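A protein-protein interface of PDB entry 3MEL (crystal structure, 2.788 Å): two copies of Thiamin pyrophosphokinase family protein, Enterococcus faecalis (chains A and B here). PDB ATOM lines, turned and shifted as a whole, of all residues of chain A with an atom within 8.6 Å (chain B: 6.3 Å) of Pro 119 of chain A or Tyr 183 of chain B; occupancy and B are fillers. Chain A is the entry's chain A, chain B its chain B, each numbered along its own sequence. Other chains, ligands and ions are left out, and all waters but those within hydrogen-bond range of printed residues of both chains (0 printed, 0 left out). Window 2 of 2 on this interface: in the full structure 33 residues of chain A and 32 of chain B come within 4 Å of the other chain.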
ATOM      1  N   GLN A  81       3.461   9.339   0.144  1.00  0.00           N
ATOM      2  CA  GLN A  81       2.541   9.194   1.273  1.00  0.00           C
ATOM      3  C   GLN A  81       1.329   8.368   0.866  1.00  0.00           C
ATOM      4  O   GLN A  81       0.890   7.475   1.592  1.00  0.00           O
ATOM      5  CB  GLN A  81       2.090  10.544   1.823  1.00  0.00           C
ATOM      6  CG  GLN A  81       3.099  11.199   2.742  1.00  0.00           C
ATOM      7  CD  GLN A  81       2.762  12.652   3.030  1.00  0.00           C
ATOM      8  OE1 GLN A  81       2.465  13.430   2.116  1.00  0.00           O
ATOM      9  NE2 GLN A  81       2.808  13.028   4.302  1.00  0.00           N
ATOM     10  N   GLN A  85       0.092   4.399   2.243  1.00  0.00           N
ATOM     11  CA  GLN A  85      -1.204   4.116   2.846  1.00  0.00           C
ATOM     12  C   GLN A  85      -1.998   3.055   2.061  1.00  0.00           C
ATOM     13  O   GLN A  85      -2.592   2.152   2.652  1.00  0.00           O
ATOM     14  CB  GLN A  85      -2.020   5.407   2.997  1.00  0.00           C
ATOM     15  CG  GLN A  85      -3.207   5.289   3.975  1.00  0.00           C
ATOM     16  CD  GLN A  85      -3.737   6.636   4.413  1.00  0.00           C
ATOM     17  OE1 GLN A  85      -3.218   7.678   4.002  1.00  0.00           O
ATOM     18  NE2 GLN A  85      -4.774   6.627   5.254  1.00  0.00           N
ATOM     19  N   TRP A 114       9.890  11.522   8.309  1.00  0.00           N
ATOM     20  CA  TRP A 114       8.987  11.780   9.423  1.00  0.00           C
ATOM     21  C   TRP A 114       7.672  11.029   9.214  1.00  0.00           C
ATOM     22  O   TRP A 114       6.679  11.302   9.881  1.00  0.00           O
ATOM     23  CB  TRP A 114       8.708  13.287   9.565  1.00  0.00           C
ATOM     24  CG  TRP A 114       9.894  14.171  10.002  1.00  0.00           C
ATOM     25  CD1 TRP A 114      10.947  13.828  10.821  1.00  0.00           C
ATOM     26  CD2 TRP A 114      10.102  15.554   9.656  1.00  0.00           C
ATOM     27  NE1 TRP A 114      11.803  14.900  10.973  1.00  0.00           N
ATOM     28  CE2 TRP A 114      11.307  15.965  10.266  1.00  0.00           C
ATOM     29  CE3 TRP A 114       9.395  16.474   8.871  1.00  0.00           C
ATOM     30  CZ2 TRP A 114      11.806  17.259  10.119  1.00  0.00           C
ATOM     31  CZ3 TRP A 114       9.899  17.744   8.723  1.00  0.00           C
ATOM     32  CH2 TRP A 114      11.086  18.131   9.348  1.00  0.00           C
ATOM     33  N   LEU A 115       7.667  10.090   8.272  1.00  0.00           N
ATOM     34  CA  LEU A 115       6.476   9.284   7.989  1.00  0.00           C
ATOM     35  C   LEU A 115       5.810   8.671   9.233  1.00  0.00           C
ATOM     36  O   LEU A 115       4.641   8.950   9.497  1.00  0.00           O
ATOM     37  CB  LEU A 115       6.775   8.235   6.923  1.00  0.00           C
ATOM     38  CG  LEU A 115       6.661   8.799   5.507  1.00  0.00           C
ATOM     39  CD1 LEU A 115       7.390   7.968   4.483  1.00  0.00           C
ATOM     40  CD2 LEU A 115       5.219   8.950   5.118  1.00  0.00           C
ATOM     41  N   PRO A 116       6.553   7.850  10.011  1.00  0.00           N
ATOM     42  CA  PRO A 116       6.080   7.267  11.276  1.00  0.00           C
ATOM     43  C   PRO A 116       5.375   8.249  12.216  1.00  0.00           C
ATOM     44  O   PRO A 116       4.574   7.815  13.041  1.00  0.00           O
ATOM     45  CB  PRO A 116       7.377   6.807  11.951  1.00  0.00           C
ATOM     46  CG  PRO A 116       8.495   7.382  11.125  1.00  0.00           C
ATOM     47  CD  PRO A 116       7.943   7.453   9.751  1.00  0.00           C
ATOM     48  N   PHE A 117       5.688   9.539  12.119  1.00  0.00           N
ATOM     49  CA  PHE A 117       5.058  10.544  12.970  1.00  0.00           C
ATOM     50  C   PHE A 117       3.576  10.667  12.700  1.00  0.00           C
ATOM     51  O   PHE A 117       2.803  10.945  13.612  1.00  0.00           O
ATOM     52  CB  PHE A 117       5.706  11.922  12.783  1.00  0.00           C
ATOM     53  CG  PHE A 117       6.899  12.159  13.663  1.00  0.00           C
ATOM     54  CD1 PHE A 117       6.810  11.973  15.023  1.00  0.00           C
ATOM     55  CD2 PHE A 117       8.098  12.577  13.128  1.00  0.00           C
ATOM     56  CE1 PHE A 117       7.894  12.163  15.822  1.00  0.00           C
ATOM     57  CE2 PHE A 117       9.182  12.785  13.931  1.00  0.00           C
ATOM     58  CZ  PHE A 117       9.080  12.577  15.280  1.00  0.00           C
ATOM     59  N   GLU A 118       3.188  10.476  11.441  1.00  0.00           N
ATOM     60  CA  GLU A 118       1.810  10.677  11.023  1.00  0.00           C
ATOM     61  C   GLU A 118       0.855   9.700  11.705  1.00  0.00           C
ATOM     62  O   GLU A 118       1.098   8.498  11.753  1.00  0.00           O
ATOM     63  CB  GLU A 118       1.718  10.551   9.514  1.00  0.00           C
ATOM     64  CG  GLU A 118       2.804  11.304   8.790  1.00  0.00           C
ATOM     65  CD  GLU A 118       2.516  11.486   7.310  1.00  0.00           C
ATOM     66  OE1 GLU A 118       1.345  11.323   6.900  1.00  0.00           O
ATOM     67  OE2 GLU A 118       3.469  11.796   6.557  1.00  0.00           O
ATOM     68  N   PRO A 119      -0.249  10.220  12.246  1.00  0.00           N
ATOM     69  CA  PRO A 119      -1.124   9.340  13.030  1.00  0.00           C
ATOM     70  C   PRO A 119      -1.534   8.097  12.252  1.00  0.00           C
ATOM     71  O   PRO A 119      -1.746   7.060  12.865  1.00  0.00           O
ATOM     72  CB  PRO A 119      -2.328  10.232  13.345  1.00  0.00           C
ATOM     73  CG  PRO A 119      -1.771  11.625  13.309  1.00  0.00           C
ATOM     74  CD  PRO A 119      -0.736  11.612  12.214  1.00  0.00           C
ATOM     75  N   ARG A 120      -1.615   8.190  10.927  1.00  0.00           N
ATOM     76  CA  ARG A 120      -1.990   7.046  10.085  1.00  0.00           C
ATOM     77  C   ARG A 120      -0.850   6.050   9.830  1.00  0.00           C
ATOM     78  O   ARG A 120      -1.048   5.065   9.145  1.00  0.00           O
ATOM     79  CB  ARG A 120      -2.543   7.525   8.738  1.00  0.00           C
ATOM     80  CG  ARG A 120      -1.469   7.794   7.708  1.00  0.00           C
ATOM     81  CD  ARG A 120      -1.970   8.649   6.552  1.00  0.00           C
ATOM     82  NE  ARG A 120      -0.901   9.471   5.987  1.00  0.00           N
ATOM     83  CZ  ARG A 120      -1.071  10.380   5.033  1.00  0.00           C
ATOM     84  NH1 ARG A 120      -2.270  10.588   4.539  1.00  0.00           N
ATOM     85  NH2 ARG A 120      -0.046  11.083   4.578  1.00  0.00           N
ATOM     86  N   PHE A 121       0.341   6.315  10.359  1.00  0.00           N
ATOM     87  CA  PHE A 121       1.493   5.441  10.166  1.00  0.00           C
ATOM     88  C   PHE A 121       2.119   5.086  11.494  1.00  0.00           C
ATOM     89  O   PHE A 121       2.893   4.137  11.578  1.00  0.00           O
ATOM     90  CB  PHE A 121       2.568   6.121   9.329  1.00  0.00           C
ATOM     91  CG  PHE A 121       2.173   6.354   7.922  1.00  0.00           C
ATOM     92  CD1 PHE A 121       1.460   5.398   7.234  1.00  0.00           C
ATOM     93  CD2 PHE A 121       2.526   7.528   7.273  1.00  0.00           C
ATOM     94  CE1 PHE A 121       1.089   5.603   5.931  1.00  0.00           C
ATOM     95  CE2 PHE A 121       2.163   7.737   5.957  1.00  0.00           C
ATOM     96  CZ  PHE A 121       1.436   6.766   5.284  1.00  0.00           C
ATOM     97  N   GLN A 122       1.832   5.881  12.518  1.00  0.00           N
ATOM     98  CA  GLN A 122       2.363   5.620  13.846  1.00  0.00           C
ATOM     99  C   GLN A 122       2.229   4.130  14.262  1.00  0.00           C
ATOM    100  O   GLN A 122       3.202   3.492  14.705  1.00  0.00           O
ATOM    101  CB  GLN A 122       1.674   6.527  14.853  1.00  0.00           C
ATOM    102  CG  GLN A 122       2.650   7.377  15.633  1.00  0.00           C
ATOM    103  CD  GLN A 122       2.458   7.251  17.132  1.00  0.00           C
ATOM    104  OE1 GLN A 122       1.371   6.883  17.602  1.00  0.00           O
ATOM    105  NE2 GLN A 122       3.511   7.554  17.897  1.00  0.00           N
ATOM    106  N   GLY A 123       1.028   3.582  14.090  1.00  0.00           N
ATOM    107  CA  GLY A 123       0.719   2.222  14.483  1.00  0.00           C
ATOM    108  C   GLY A 123       1.554   1.180  13.775  1.00  0.00           C
ATOM    109  O   GLY A 123       1.550   0.009  14.157  1.00  0.00           O
ATOM    110  N   VAL A 124       2.285   1.596  12.751  1.00  0.00           N
ATOM    111  CA  VAL A 124       3.171   0.682  12.051  1.00  0.00           C
ATOM    112  C   VAL A 124       4.593   1.225  11.825  1.00  0.00           C
ATOM    113  O   VAL A 124       5.185   0.952  10.779  1.00  0.00           O
ATOM    114  CB  VAL A 124       2.563   0.223  10.694  1.00  0.00           C
ATOM    115  CG1 VAL A 124       1.228  -0.482  10.906  1.00  0.00           C
ATOM    116  CG2 VAL A 124       2.394   1.393   9.735  1.00  0.00           C
ATOM    117  N   LEU A 125       5.152   1.967  12.784  1.00  0.00           N
ATOM    118  CA  LEU A 125       6.504   2.518  12.601  1.00  0.00           C
ATOM    119  C   LEU A 125       7.553   1.429  12.513  1.00  0.00           C
ATOM    120  O   LEU A 125       8.561   1.549  11.820  1.00  0.00           O
ATOM    121  CB  LEU A 125       6.875   3.484  13.724  1.00  0.00           C
ATOM    122  CG  LEU A 125       6.872   3.026  15.177  1.00  0.00           C
ATOM    123  CD1 LEU A 125       8.174   2.401  15.576  1.00  0.00           C
ATOM    124  CD2 LEU A 125       6.609   4.239  16.025  1.00  0.00           C
ATOM    125  N   LEU A 161      14.762  11.782  16.608  1.00  0.00           N
ATOM    126  CA  LEU A 161      13.970  12.709  15.828  1.00  0.00           C
ATOM    127  C   LEU A 161      13.292  13.730  16.742  1.00  0.00           C
ATOM    128  O   LEU A 161      12.902  14.843  16.313  1.00  0.00           O
ATOM    129  CB  LEU A 161      12.955  11.949  14.987  1.00  0.00           C
ATOM    130  CG  LEU A 161      13.610  10.947  14.041  1.00  0.00           C
ATOM    131  CD1 LEU A 161      12.541  10.144  13.312  1.00  0.00           C
ATOM    132  CD2 LEU A 161      14.555  11.662  13.072  1.00  0.00           C
ATOM    133  N   THR A 162      13.183  13.351  18.008  1.00  0.00           N
ATOM    134  CA  THR A 162      12.571  14.189  19.011  1.00  0.00           C
ATOM    135  C   THR A 162      13.443  14.158  20.240  1.00  0.00           C
ATOM    136  O   THR A 162      14.304  13.297  20.357  1.00  0.00           O
ATOM    137  CB  THR A 162      11.255  13.596  19.439  1.00  0.00           C
ATOM    138  OG1 THR A 162      11.521  12.372  20.126  1.00  0.00           O
ATOM    139  CG2 THR A 162      10.379  13.341  18.236  1.00  0.00           C
ATOM    140  N   CYS B 160       8.954  21.907   9.690  1.00  0.00           N
ATOM    141  CA  CYS B 160       8.972  22.066  11.127  1.00  0.00           C
ATOM    142  C   CYS B 160       9.772  20.935  11.792  1.00  0.00           C
ATOM    143  O   CYS B 160       9.303  19.814  11.913  1.00  0.00           O
ATOM    144  CB  CYS B 160       7.548  22.097  11.663  1.00  0.00           C
ATOM    145  SG  CYS B 160       6.441  23.191  10.751  1.00  0.00           S
ATOM    146  N   THR B 162      10.297  20.622  14.678  1.00  0.00           N
ATOM    147  CA  THR B 162       9.690  20.325  15.975  1.00  0.00           C
ATOM    148  C   THR B 162       8.208  20.630  15.885  1.00  0.00           C
ATOM    149  O   THR B 162       7.773  21.253  14.925  1.00  0.00           O
ATOM    150  CB  THR B 162      10.258  21.218  17.091  1.00  0.00           C
ATOM    151  OG1 THR B 162      10.116  22.590  16.702  1.00  0.00           O
ATOM    152  CG2 THR B 162      11.706  20.922  17.340  1.00  0.00           C
ATOM    153  N   PRO B 163       7.427  20.200  16.887  1.00  0.00           N
ATOM    154  CA  PRO B 163       6.044  20.676  16.939  1.00  0.00           C
ATOM    155  C   PRO B 163       6.028  22.196  16.880  1.00  0.00           C
ATOM    156  O   PRO B 163       6.769  22.855  17.618  1.00  0.00           O
ATOM    157  CB  PRO B 163       5.559  20.201  18.309  1.00  0.00           C
ATOM    158  CG  PRO B 163       6.367  19.034  18.603  1.00  0.00           C
ATOM    159  CD  PRO B 163       7.708  19.217  17.942  1.00  0.00           C
ATOM    160  N   VAL B 164       5.207  22.739  15.991  1.00  0.00           N
ATOM    161  CA  VAL B 164       5.123  24.180  15.784  1.00  0.00           C
ATOM    162  C   VAL B 164       3.733  24.714  16.117  1.00  0.00           C
ATOM    163  O   VAL B 164       2.732  24.056  15.835  1.00  0.00           O
ATOM    164  CB  VAL B 164       5.495  24.537  14.348  1.00  0.00           C
ATOM    165  CG1 VAL B 164       4.971  25.903  13.992  1.00  0.00           C
ATOM    166  CG2 VAL B 164       7.015  24.452  14.167  1.00  0.00           C
ATOM    167  N   VAL B 181       1.127  22.423  14.203  1.00  0.00           N
ATOM    168  CA  VAL B 181       1.928  21.298  13.704  1.00  0.00           C
ATOM    169  C   VAL B 181       2.416  20.478  14.882  1.00  0.00           C
ATOM    170  O   VAL B 181       3.420  20.810  15.479  1.00  0.00           O
ATOM    171  CB  VAL B 181       3.148  21.788  12.913  1.00  0.00           C
ATOM    172  CG1 VAL B 181       3.826  20.639  12.202  1.00  0.00           C
ATOM    173  CG2 VAL B 181       2.738  22.847  11.920  1.00  0.00           C
ATOM    174  N   PRO B 182       1.699  19.404  15.228  1.00  0.00           N
ATOM    175  CA  PRO B 182       1.892  18.681  16.499  1.00  0.00           C
ATOM    176  C   PRO B 182       3.142  17.800  16.570  1.00  0.00           C
ATOM    177  O   PRO B 182       3.583  17.475  17.674  1.00  0.00           O
ATOM    178  CB  PRO B 182       0.641  17.791  16.601  1.00  0.00           C
ATOM    179  CG  PRO B 182      -0.285  18.243  15.495  1.00  0.00           C
ATOM    180  CD  PRO B 182       0.592  18.846  14.440  1.00  0.00           C
ATOM    181  N   TYR B 183       3.675  17.407  15.418  1.00  0.00           N
ATOM    182  CA  TYR B 183       4.857  16.558  15.329  1.00  0.00           C
ATOM    183  C   TYR B 183       5.606  17.086  14.109  1.00  0.00           C
ATOM    184  O   TYR B 183       5.049  17.851  13.336  1.00  0.00           O
ATOM    185  CB  TYR B 183       4.435  15.094  15.136  1.00  0.00           C
ATOM    186  CG  TYR B 183       3.279  14.954  14.164  1.00  0.00           C
ATOM    187  CD1 TYR B 183       3.506  14.943  12.794  1.00  0.00           C
ATOM    188  CD2 TYR B 183       1.960  14.885  14.612  1.00  0.00           C
ATOM    189  CE1 TYR B 183       2.468  14.861  11.894  1.00  0.00           C
ATOM    190  CE2 TYR B 183       0.906  14.798  13.709  1.00  0.00           C
ATOM    191  CZ  TYR B 183       1.171  14.789  12.348  1.00  0.00           C
ATOM    192  OH  TYR B 183       0.167  14.708  11.408  1.00  0.00           O
ATOM    193  N   PRO B 184       6.874  16.699  13.926  1.00  0.00           N
ATOM    194  CA  PRO B 184       7.590  17.252  12.773  1.00  0.00           C
ATOM    195  C   PRO B 184       6.896  16.977  11.439  1.00  0.00           C
ATOM    196  O   PRO B 184       6.635  15.835  11.101  1.00  0.00           O
ATOM    197  CB  PRO B 184       8.944  16.554  12.843  1.00  0.00           C
ATOM    198  CG  PRO B 184       9.115  16.266  14.291  1.00  0.00           C
ATOM    199  CD  PRO B 184       7.764  15.938  14.813  1.00  0.00           C
ATOM    200  N   THR B 185       6.604  18.031  10.693  1.00  0.00           N
ATOM    201  CA  THR B 185       5.887  17.918   9.432  1.00  0.00           C
ATOM    202  C   THR B 185       6.644  18.723   8.396  1.00  0.00           C
ATOM    203  O   THR B 185       7.219  19.740   8.718  1.00  0.00           O
ATOM    204  CB  THR B 185       4.456  18.482   9.555  1.00  0.00           C
ATOM    205  OG1 THR B 185       3.723  17.756  10.550  1.00  0.00           O
ATOM    206  CG2 THR B 185       3.724  18.404   8.230  1.00  0.00           C
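Hydrophobic or aromatic side chains of chain A within 4 Å of the printed part of chain B: Trp 114, Phe 117 and Pro 119.
Of the 9 printed residues of chain B, 4 touch a printed residue of chain A.
Hydrophobic or aromatic side chains of chain B within 4 Å of the printed part of chain A: Tyr 183 and Pro 184.
Among the printed residues, no Asp or Glu carboxylate lies within 4 Å of a Lys or Arg side-chain nitrogen of the other chain.
Position printed for both chains: 162.
Among the printed residues, pairs that only touch across the chains: Trp 114 of chain A with Cys 160 of chain B, Trp 114 of chain A with Pro 184 of chain B, Trp 114 of chain A with Thr 185 of chain B, Phe 117 of chain A with Tyr 183 of chain B, Phe 117 of chain A with Pro 184 of chain B and Pro 119 of chain A with Tyr 183 of chain B.
The backbone NH (N) of Cys 160 of chain B lies within hydrogen-bond range of the backbone carbonyl oxygen (O) of Thr 185 of chain B (2.9 Å).
The backbone carbonyl oxygen (O) of Tyr 183 of chain B is in hydrogen-bond range of the side-chain hydroxyl (OG1) of Thr 185 of chain B (3.1 Å).
Of the printed residues of chain B, Trp 114 of chain A touches Cys 160, Pro 184 and Thr 185.
Printed residues of chain B within 4 Å of Phe 117 of chain A: Tyr 183 (3.7 Å) and Pro 184 (3.5 Å).
Pro 119 of chain A touches one residue of chain B.
Printed residues of chain A within 4 Å of Cys 160 of chain B: Trp 114 (3.5 Å).
No residue of chain A comes within 4 Å of Pro 182 of chain B.
Tyr 183 of chain B touches just these residues of chain A: Phe 117 and Pro 119.
Printed residues of chain A within 4 Å of Thr 185 of chain B: Trp 114 (3.3 Å).
The nearest printed residue of chain A that does not touch Cys 160 of chain B is Phe 117 of chain A (7.3 Å).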
